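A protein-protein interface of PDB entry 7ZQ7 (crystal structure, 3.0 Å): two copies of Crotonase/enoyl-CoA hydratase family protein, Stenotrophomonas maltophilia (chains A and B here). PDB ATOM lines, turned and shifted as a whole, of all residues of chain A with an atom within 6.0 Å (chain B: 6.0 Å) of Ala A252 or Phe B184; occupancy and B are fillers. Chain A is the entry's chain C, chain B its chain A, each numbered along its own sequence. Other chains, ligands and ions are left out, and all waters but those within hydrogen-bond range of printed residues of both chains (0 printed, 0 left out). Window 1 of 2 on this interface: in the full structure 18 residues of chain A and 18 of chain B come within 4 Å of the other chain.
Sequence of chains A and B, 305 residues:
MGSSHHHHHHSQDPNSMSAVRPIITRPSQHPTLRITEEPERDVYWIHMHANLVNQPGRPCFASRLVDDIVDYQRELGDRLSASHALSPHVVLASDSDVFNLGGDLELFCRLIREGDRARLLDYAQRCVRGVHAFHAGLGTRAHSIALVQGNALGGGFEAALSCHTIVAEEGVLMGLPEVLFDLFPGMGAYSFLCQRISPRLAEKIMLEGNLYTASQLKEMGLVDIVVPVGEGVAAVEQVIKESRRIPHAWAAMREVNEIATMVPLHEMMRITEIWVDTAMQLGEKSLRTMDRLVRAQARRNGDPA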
ATOM      1  N   ARG A 141     -15.958  -7.697  22.983  1.00  0.00           N
ATOM      2  CA  ARG A 141     -14.978  -8.393  23.864  1.00  0.00           C
ATOM      3  C   ARG A 141     -15.631  -8.658  25.224  1.00  0.00           C
ATOM      4  O   ARG A 141     -14.952  -8.488  26.257  1.00  0.00           O
ATOM      5  CB  ARG A 141     -13.645  -7.640  23.958  1.00  0.00           C
ATOM      6  CG  ARG A 141     -13.116  -7.141  22.621  1.00  0.00           C
ATOM      7  CD  ARG A 141     -11.674  -7.546  22.383  1.00  0.00           C
ATOM      8  NE  ARG A 141     -11.259  -7.334  21.004  1.00  0.00           N
ATOM      9  CZ  ARG A 141     -10.684  -6.225  20.553  1.00  0.00           C
ATOM     10  NH1 ARG A 141     -10.452  -5.218  21.378  1.00  0.00           N
ATOM     11  NH2 ARG A 141     -10.344  -6.126  19.281  1.00  0.00           N
ATOM     12  N   PRO A 247     -10.305  -6.082  34.078  1.00  0.00           N
ATOM     13  CA  PRO A 247     -10.895  -5.740  32.766  1.00  0.00           C
ATOM     14  C   PRO A 247      -9.897  -5.683  31.617  1.00  0.00           C
ATOM     15  O   PRO A 247     -10.220  -6.162  30.527  1.00  0.00           O
ATOM     16  CB  PRO A 247     -11.515  -4.353  32.996  1.00  0.00           C
ATOM     17  CG  PRO A 247     -10.861  -3.812  34.238  1.00  0.00           C
ATOM     18  CD  PRO A 247     -10.328  -4.963  35.036  1.00  0.00           C
ATOM     19  N   HIS A 248      -8.705  -5.098  31.805  1.00  0.00           N
ATOM     20  CA  HIS A 248      -7.836  -4.832  30.655  1.00  0.00           C
ATOM     21  C   HIS A 248      -7.194  -6.113  30.088  1.00  0.00           C
ATOM     22  O   HIS A 248      -7.006  -6.237  28.861  1.00  0.00           O
ATOM     23  CB  HIS A 248      -6.760  -3.811  31.042  1.00  0.00           C
ATOM     24  CG  HIS A 248      -7.227  -2.388  31.007  1.00  0.00           C
ATOM     25  ND1 HIS A 248      -7.724  -1.744  32.118  1.00  0.00           N
ATOM     26  CD2 HIS A 248      -7.237  -1.474  30.007  1.00  0.00           C
ATOM     27  CE1 HIS A 248      -8.047  -0.503  31.799  1.00  0.00           C
ATOM     28  NE2 HIS A 248      -7.759  -0.312  30.525  1.00  0.00           N
ATOM     29  N   ALA A 249      -6.847  -7.067  30.960  1.00  0.00           N
ATOM     30  CA  ALA A 249      -6.293  -8.334  30.501  1.00  0.00           C
ATOM     31  C   ALA A 249      -7.329  -9.147  29.732  1.00  0.00           C
ATOM     32  O   ALA A 249      -6.999  -9.810  28.734  1.00  0.00           O
ATOM     33  CB  ALA A 249      -5.769  -9.132  31.692  1.00  0.00           C
ATOM     34  N   TRP A 250      -8.582  -9.139  30.203  1.00  0.00           N
ATOM     35  CA  TRP A 250      -9.612  -9.851  29.471  1.00  0.00           C
ATOM     36  C   TRP A 250      -9.732  -9.312  28.055  1.00  0.00           C
ATOM     37  O   TRP A 250      -9.809 -10.085  27.093  1.00  0.00           O
ATOM     38  CB  TRP A 250     -10.958  -9.766  30.183  1.00  0.00           C
ATOM     39  CG  TRP A 250     -11.940 -10.666  29.492  1.00  0.00           C
ATOM     40  CD1 TRP A 250     -12.782 -10.337  28.459  1.00  0.00           C
ATOM     41  CD2 TRP A 250     -12.126 -12.066  29.729  1.00  0.00           C
ATOM     42  NE1 TRP A 250     -13.504 -11.437  28.068  1.00  0.00           N
ATOM     43  CE2 TRP A 250     -13.117 -12.515  28.825  1.00  0.00           C
ATOM     44  CE3 TRP A 250     -11.569 -12.978  30.631  1.00  0.00           C
ATOM     45  CZ2 TRP A 250     -13.553 -13.845  28.793  1.00  0.00           C
ATOM     46  CZ3 TRP A 250     -12.000 -14.285  30.603  1.00  0.00           C
ATOM     47  CH2 TRP A 250     -12.980 -14.712  29.687  1.00  0.00           C
ATOM     48  N   ALA A 251      -9.727  -7.990  27.899  1.00  0.00           N
ATOM     49  CA  ALA A 251      -9.850  -7.429  26.561  1.00  0.00           C
ATOM     50  C   ALA A 251      -8.657  -7.817  25.702  1.00  0.00           C
ATOM     51  O   ALA A 251      -8.820  -8.249  24.560  1.00  0.00           O
ATOM     52  CB  ALA A 251      -9.997  -5.914  26.638  1.00  0.00           C
ATOM     53  N   ALA A 252      -7.444  -7.680  26.239  1.00  0.00           N
ATOM     54  CA  ALA A 252      -6.263  -8.088  25.481  1.00  0.00           C
ATOM     55  C   ALA A 252      -6.348  -9.561  25.074  1.00  0.00           C
ATOM     56  O   ALA A 252      -6.263  -9.887  23.886  1.00  0.00           O
ATOM     57  CB  ALA A 252      -4.996  -7.814  26.291  1.00  0.00           C
ATOM     58  N   MET A 253      -6.547 -10.467  26.044  1.00  0.00           N
ATOM     59  CA  MET A 253      -6.613 -11.890  25.706  1.00  0.00           C
ATOM     60  C   MET A 253      -7.753 -12.184  24.754  1.00  0.00           C
ATOM     61  O   MET A 253      -7.636 -13.064  23.902  1.00  0.00           O
ATOM     62  CB  MET A 253      -6.760 -12.752  26.957  1.00  0.00           C
ATOM     63  CG  MET A 253      -5.422 -13.176  27.512  1.00  0.00           C
ATOM     64  SD  MET A 253      -4.142 -13.754  26.339  1.00  0.00           S
ATOM     65  CE  MET A 253      -4.991 -14.770  25.092  1.00  0.00           C
ATOM     66  N   ARG A 254      -8.866 -11.472  24.892  1.00  0.00           N
ATOM     67  CA  ARG A 254      -9.943 -11.593  23.921  1.00  0.00           C
ATOM     68  C   ARG A 254      -9.433 -11.277  22.516  1.00  0.00           C
ATOM     69  O   ARG A 254      -9.723 -12.005  21.569  1.00  0.00           O
ATOM     70  CB  ARG A 254     -11.095 -10.671  24.357  1.00  0.00           C
ATOM     71  CG  ARG A 254     -12.496 -11.006  23.893  1.00  0.00           C
ATOM     72  CD  ARG A 254     -12.881 -12.436  24.157  1.00  0.00           C
ATOM     73  NE  ARG A 254     -12.282 -13.009  25.351  1.00  0.00           N
ATOM     74  CZ  ARG A 254     -11.739 -14.220  25.420  1.00  0.00           C
ATOM     75  NH1 ARG A 254     -11.616 -15.002  24.351  1.00  0.00           N
ATOM     76  NH2 ARG A 254     -11.316 -14.667  26.595  1.00  0.00           N
ATOM     77  N   GLU A 255      -8.612 -10.234  22.381  1.00  0.00           N
ATOM     78  CA  GLU A 255      -8.169  -9.786  21.061  1.00  0.00           C
ATOM     79  C   GLU A 255      -7.106 -10.722  20.491  1.00  0.00           C
ATOM     80  O   GLU A 255      -7.055 -10.956  19.272  1.00  0.00           O
ATOM     81  CB  GLU A 255      -7.633  -8.351  21.152  1.00  0.00           C
ATOM     82  CG  GLU A 255      -7.023  -7.810  19.875  1.00  0.00           C
ATOM     83  CD  GLU A 255      -6.844  -6.288  19.879  1.00  0.00           C
ATOM     84  OE1 GLU A 255      -6.425  -5.724  18.827  1.00  0.00           O
ATOM     85  OE2 GLU A 255      -7.125  -5.652  20.926  1.00  0.00           O
ATOM     86  N   VAL A 256      -6.241 -11.255  21.357  1.00  0.00           N
ATOM     87  CA  VAL A 256      -5.251 -12.214  20.898  1.00  0.00           C
ATOM     88  C   VAL A 256      -5.947 -13.430  20.302  1.00  0.00           C
ATOM     89  O   VAL A 256      -5.522 -13.962  19.268  1.00  0.00           O
ATOM     90  CB  VAL A 256      -4.286 -12.594  22.038  1.00  0.00           C
ATOM     91  CG1 VAL A 256      -3.087 -13.316  21.470  1.00  0.00           C
ATOM     92  CG2 VAL A 256      -3.807 -11.358  22.759  1.00  0.00           C
ATOM     93  N   ASN A 257      -7.044 -13.868  20.900  1.00  0.00           N
ATOM     94  CA  ASN A 257      -7.724 -15.060  20.339  1.00  0.00           C
ATOM     95  C   ASN A 257      -8.361 -14.695  19.003  1.00  0.00           C
ATOM     96  O   ASN A 257      -8.905 -15.572  18.350  1.00  0.00           O
ATOM     97  CB  ASN A 257      -8.759 -15.634  21.296  1.00  0.00           C
ATOM     98  CG  ASN A 257      -8.170 -16.676  22.209  1.00  0.00           C
ATOM     99  OD1 ASN A 257      -7.464 -17.567  21.762  1.00  0.00           O
ATOM    100  ND2 ASN A 257      -8.442 -16.557  23.490  1.00  0.00           N
ATOM    101  N   GLU B 178       1.431 -11.879  35.873  1.00  0.00           N
ATOM    102  CA  GLU B 178       1.287 -10.587  35.211  1.00  0.00           C
ATOM    103  C   GLU B 178      -0.147 -10.047  35.282  1.00  0.00           C
ATOM    104  O   GLU B 178      -0.351  -8.862  34.990  1.00  0.00           O
ATOM    105  CB  GLU B 178       1.777 -10.690  33.745  1.00  0.00           C
ATOM    106  CG  GLU B 178       3.272 -11.191  33.522  1.00  0.00           C
ATOM    107  CD  GLU B 178       4.276 -10.072  33.036  1.00  0.00           C
ATOM    108  OE1 GLU B 178       5.485 -10.099  33.421  1.00  0.00           O
ATOM    109  OE2 GLU B 178       3.863  -9.163  32.264  1.00  0.00           O
ATOM    110  N   VAL B 179      -1.133 -10.865  35.685  1.00  0.00           N
ATOM    111  CA  VAL B 179      -2.520 -10.403  35.846  1.00  0.00           C
ATOM    112  C   VAL B 179      -2.744  -9.596  37.124  1.00  0.00           C
ATOM    113  O   VAL B 179      -3.731  -8.845  37.211  1.00  0.00           O
ATOM    114  CB  VAL B 179      -3.521 -11.576  35.813  1.00  0.00           C
ATOM    115  CG1 VAL B 179      -3.278 -12.437  34.650  1.00  0.00           C
ATOM    116  CG2 VAL B 179      -3.380 -12.419  37.059  1.00  0.00           C
ATOM    117  N   PHE B 181      -1.466  -6.974  38.051  1.00  0.00           N
ATOM    118  CA  PHE B 181      -1.674  -5.568  37.726  1.00  0.00           C
ATOM    119  C   PHE B 181      -2.612  -5.367  36.542  1.00  0.00           C
ATOM    120  O   PHE B 181      -2.561  -4.313  35.900  1.00  0.00           O
ATOM    121  CB  PHE B 181      -0.350  -4.831  37.486  1.00  0.00           C
ATOM    122  CG  PHE B 181       0.740  -5.662  36.872  1.00  0.00           C
ATOM    123  CD1 PHE B 181       1.509  -6.531  37.649  1.00  0.00           C
ATOM    124  CD2 PHE B 181       1.019  -5.544  35.516  1.00  0.00           C
ATOM    125  CE1 PHE B 181       2.532  -7.270  37.075  1.00  0.00           C
ATOM    126  CE2 PHE B 181       2.030  -6.291  34.923  1.00  0.00           C
ATOM    127  CZ  PHE B 181       2.798  -7.156  35.700  1.00  0.00           C
ATOM    128  N   ASP B 182      -3.500  -6.333  36.271  1.00  0.00           N
ATOM    129  CA  ASP B 182      -4.464  -6.238  35.166  1.00  0.00           C
ATOM    130  C   ASP B 182      -3.730  -6.106  33.830  1.00  0.00           C
ATOM    131  O   ASP B 182      -4.080  -5.293  32.971  1.00  0.00           O
ATOM    132  CB  ASP B 182      -5.460  -5.087  35.396  1.00  0.00           C
ATOM    133  CG  ASP B 182      -6.539  -4.977  34.299  1.00  0.00           C
ATOM    134  OD1 ASP B 182      -7.081  -6.006  33.852  1.00  0.00           O
ATOM    135  OD2 ASP B 182      -6.856  -3.839  33.894  1.00  0.00           O
ATOM    136  N   LEU B 183      -2.665  -6.891  33.677  1.00  0.00           N
ATOM    137  CA  LEU B 183      -1.957  -7.097  32.424  1.00  0.00           C
ATOM    138  C   LEU B 183      -1.872  -8.596  32.200  1.00  0.00           C
ATOM    139  O   LEU B 183      -2.233  -9.400  33.065  1.00  0.00           O
ATOM    140  CB  LEU B 183      -0.548  -6.495  32.444  1.00  0.00           C
ATOM    141  CG  LEU B 183      -0.150  -5.496  31.370  1.00  0.00           C
ATOM    142  CD1 LEU B 183       1.332  -5.288  31.465  1.00  0.00           C
ATOM    143  CD2 LEU B 183      -0.512  -5.999  30.011  1.00  0.00           C
ATOM    144  N   PHE B 184      -1.386  -8.977  31.033  1.00  0.00           N
ATOM    145  CA  PHE B 184      -1.240 -10.380  30.683  1.00  0.00           C
ATOM    146  C   PHE B 184       0.165 -10.620  30.156  1.00  0.00           C
ATOM    147  O   PHE B 184       0.848  -9.681  29.729  1.00  0.00           O
ATOM    148  CB  PHE B 184      -2.298 -10.793  29.649  1.00  0.00           C
ATOM    149  CG  PHE B 184      -1.912 -10.472  28.259  1.00  0.00           C
ATOM    150  CD1 PHE B 184      -2.102  -9.190  27.764  1.00  0.00           C
ATOM    151  CD2 PHE B 184      -1.316 -11.442  27.450  1.00  0.00           C
ATOM    152  CE1 PHE B 184      -1.732  -8.879  26.477  1.00  0.00           C
ATOM    153  CE2 PHE B 184      -0.945 -11.142  26.171  1.00  0.00           C
ATOM    154  CZ  PHE B 184      -1.150  -9.855  25.677  1.00  0.00           C
ATOM    155  N   PRO B 185       0.635 -11.861  30.191  1.00  0.00           N
ATOM    156  CA  PRO B 185       2.000 -12.140  29.739  1.00  0.00           C
ATOM    157  C   PRO B 185       2.062 -12.160  28.225  1.00  0.00           C
ATOM    158  O   PRO B 185       1.672 -13.171  27.642  1.00  0.00           O
ATOM    159  CB  PRO B 185       2.282 -13.535  30.317  1.00  0.00           C
ATOM    160  CG  PRO B 185       1.069 -13.881  31.167  1.00  0.00           C
ATOM    161  CD  PRO B 185      -0.050 -13.103  30.575  1.00  0.00           C
ATOM    162  N   GLY B 186       2.523 -11.085  27.578  1.00  0.00           N
ATOM    163  CA  GLY B 186       2.545 -10.990  26.132  1.00  0.00           C
ATOM    164  C   GLY B 186       3.888 -11.240  25.471  1.00  0.00           C
ATOM    165  O   GLY B 186       4.006 -11.122  24.247  1.00  0.00           O
ATOM    166  N   MET B 187       4.900 -11.563  26.282  1.00  0.00           N
ATOM    167  CA  MET B 187       6.271 -11.821  25.763  1.00  0.00           C
ATOM    168  C   MET B 187       6.221 -12.947  24.723  1.00  0.00           C
ATOM    169  O   MET B 187       6.710 -12.735  23.596  1.00  0.00           O
ATOM    170  CB  MET B 187       7.219 -12.221  26.898  1.00  0.00           C
ATOM    171  CG  MET B 187       8.549 -11.491  26.859  1.00  0.00           C
ATOM    172  SD  MET B 187       9.774 -12.217  27.977  1.00  0.00           S
ATOM    173  CE  MET B 187       9.685 -11.072  29.352  1.00  0.00           C
ATOM    174  N   MET B 206      -2.943 -18.414  32.167  1.00  0.00           N
ATOM    175  CA  MET B 206      -2.441 -17.048  32.035  1.00  0.00           C
ATOM    176  C   MET B 206      -3.183 -16.087  32.960  1.00  0.00           C
ATOM    177  O   MET B 206      -2.553 -15.312  33.697  1.00  0.00           O
ATOM    178  CB  MET B 206      -2.570 -16.563  30.596  1.00  0.00           C
ATOM    179  CG  MET B 206      -1.833 -17.352  29.530  1.00  0.00           C
ATOM    180  SD  MET B 206      -1.365 -16.284  28.147  1.00  0.00           S
ATOM    181  CE  MET B 206      -2.545 -16.852  26.974  1.00  0.00           C
ATOM    182  N   LEU B 207      -4.530 -16.122  32.918  1.00  0.00           N
ATOM    183  CA  LEU B 207      -5.404 -15.182  33.620  1.00  0.00           C
ATOM    184  C   LEU B 207      -5.669 -15.566  35.067  1.00  0.00           C
ATOM    185  O   LEU B 207      -5.761 -14.671  35.918  1.00  0.00           O
ATOM    186  CB  LEU B 207      -6.745 -15.030  32.889  1.00  0.00           C
ATOM    187  CG  LEU B 207      -6.686 -14.346  31.518  1.00  0.00           C
ATOM    188  CD1 LEU B 207      -7.970 -13.619  31.220  1.00  0.00           C
ATOM    189  CD2 LEU B 207      -5.494 -13.382  31.406  1.00  0.00           C
ATOM    190  N   ILE B 271       1.050  -9.880  18.931  1.00  0.00           N
ATOM    191  CA  ILE B 271       0.571 -10.071  20.292  1.00  0.00           C
ATOM    192  C   ILE B 271       1.152  -9.011  21.223  1.00  0.00           C
ATOM    193  O   ILE B 271       0.421  -8.403  22.013  1.00  0.00           O
ATOM    194  CB  ILE B 271       0.879 -11.499  20.770  1.00  0.00           C
ATOM    195  CG1 ILE B 271       0.094 -12.508  19.915  1.00  0.00           C
ATOM    196  CG2 ILE B 271       0.562 -11.628  22.290  1.00  0.00           C
ATOM    197  CD1 ILE B 271       0.122 -13.923  20.434  1.00  0.00           C
ATOM    198  N   THR B 272       2.459  -8.732  21.124  1.00  0.00           N
ATOM    199  CA  THR B 272       3.016  -7.698  21.999  1.00  0.00           C
ATOM    200  C   THR B 272       2.484  -6.315  21.655  1.00  0.00           C
ATOM    201  O   THR B 272       2.278  -5.495  22.556  1.00  0.00           O
ATOM    202  CB  THR B 272       4.542  -7.687  21.958  1.00  0.00           C
ATOM    203  OG1 THR B 272       4.984  -7.281  20.660  1.00  0.00           O
ATOM    204  CG2 THR B 272       5.088  -9.037  22.311  1.00  0.00           C
ATOM    205  N   ILE B 274      -0.457  -5.760  21.027  1.00  0.00           N
ATOM    206  CA  ILE B 274      -1.650  -5.675  21.858  1.00  0.00           C
ATOM    207  C   ILE B 274      -1.259  -5.410  23.305  1.00  0.00           C
ATOM    208  O   ILE B 274      -1.841  -4.551  23.976  1.00  0.00           O
ATOM    209  CB  ILE B 274      -2.491  -6.955  21.747  1.00  0.00           C
ATOM    210  CG1 ILE B 274      -3.147  -7.076  20.382  1.00  0.00           C
ATOM    211  CG2 ILE B 274      -3.549  -6.989  22.846  1.00  0.00           C
ATOM    212  CD1 ILE B 274      -3.592  -8.492  20.100  1.00  0.00           C
ATOM    213  N   TRP B 275      -0.282  -6.169  23.808  1.00  0.00           N
ATOM    214  CA  TRP B 275       0.225  -5.971  25.162  1.00  0.00           C
ATOM    215  C   TRP B 275       0.653  -4.527  25.395  1.00  0.00           C
ATOM    216  O   TRP B 275       0.385  -3.957  26.461  1.00  0.00           O
ATOM    217  CB  TRP B 275       1.398  -6.917  25.399  1.00  0.00           C
ATOM    218  CG  TRP B 275       2.063  -6.918  26.783  1.00  0.00           C
ATOM    219  CD1 TRP B 275       1.765  -7.746  27.840  1.00  0.00           C
ATOM    220  CD2 TRP B 275       3.178  -6.120  27.211  1.00  0.00           C
ATOM    221  NE1 TRP B 275       2.602  -7.499  28.896  1.00  0.00           N
ATOM    222  CE2 TRP B 275       3.479  -6.505  28.543  1.00  0.00           C
ATOM    223  CE3 TRP B 275       3.939  -5.110  26.608  1.00  0.00           C
ATOM    224  CZ2 TRP B 275       4.515  -5.908  29.282  1.00  0.00           C
ATOM    225  CZ3 TRP B 275       4.964  -4.521  27.341  1.00  0.00           C
ATOM    226  CH2 TRP B 275       5.243  -4.924  28.663  1.00  0.00           C
ATOM    227  N   THR B 278      -2.410  -2.342  25.729  1.00  0.00           N
ATOM    228  CA  THR B 278      -3.071  -2.595  26.999  1.00  0.00           C
ATOM    229  C   THR B 278      -2.354  -1.882  28.126  1.00  0.00           C
ATOM    230  O   THR B 278      -2.957  -1.103  28.863  1.00  0.00           O
ATOM    231  CB  THR B 278      -3.109  -4.088  27.282  1.00  0.00           C
ATOM    232  OG1 THR B 278      -4.176  -4.680  26.543  1.00  0.00           O
ATOM    233  CG2 THR B 278      -3.373  -4.315  28.748  1.00  0.00           C
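Of the printed residues of chain B, His A248 touches Asp B182 (2.8 Å) and Thr B278 (3.98 Å). Printed residues of chain B within 4 Å of Ala A249: Asp B182 (3.1 Å) and Leu B183 (3.8 Å). Ala A252 touches just these residues of chain B: Phe B184, Ile B274 and Thr B278. Of the printed residues of chain B, Met A253 touches Phe B184, Met B206 and Leu B207. Of the printed residues of chain A, Met B206 touches Met A253. Thr B272 touches none of the printed residues of chain A. Printed residues of chain A within 4 Å of Ile B274: Ala A252 (3.8 Å), Glu A255 (3.5 Å) and Val A256 (3.9 Å). The nearest residue of chain B that does not touch Ala A252 is Trp B275 (5.6 Å). The nearest printed residue of chain B that does not touch Ala A249 is Leu B207 (4.3 Å).
Among the printed residues, merely in contact across the chains: Ala A252 with Thr B278 (3.2 Å), Val A256 with Ile B271 (3.4 Å), Ala A252 with Phe B184 (3.4 Å), Glu A255 with Ile B274 (3.5 Å), Met A253 with Met B206 (3.5 Å), Trp A250 with Leu B207 (3.7 Å), Ala A249 with Leu B183 (3.8 Å), Met A253 with Phe B184 (3.8 Å), Ala A252 with Ile B274 (3.8 Å), Met A253 with Leu B207 (3.9 Å), Val A256 with Ile B274 (3.9 Å) and His A248 with Thr B278 (3.98 Å).
The backbone carbonyl oxygen (O) of Glu B178 sits close to the backbone NH (N) of Leu B183 (3.3 Å). O of Phe B184 sits close to NE1 of Trp B275. The backbone carbonyl oxygen (O) of Ile B274 is in hydrogen-bond range of the side-chain hydroxyl (OG1) of Thr B278 (3.5 Å). The guanidinium group (NH1) of Arg A141 is in salt-bridge range of the side-chain carboxylate (OE2) of Glu A255, 3.4 Å away.
No position is printed for both chains. Of the 15 pairs that touch across the chains among the printed residues, none has its exchanged pair printed and touching as well.
N of His A248 sits at hydrogen-bond distance from OD1 of Asp B182, at 2.8 Å. OD1 of Asp B182 sits at hydrogen-bond distance from N of Ala A249 (3.1 Å). N of Pro A247 sits close to OD1 of Asp B182.
Along chain B the printed residues that touch a printed residue of chain A span positions 182 to 278. Hydrophobic or aromatic side chains of chain A that line the printed part of chain B: Pro A247, His A248, Ala A249, Trp A250, Ala A252, Met A253 and Val A256. Among the printed residues, no Asp or Glu carboxylate lies within 4 Å of a Lys or Arg side-chain nitrogen of the other chain.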
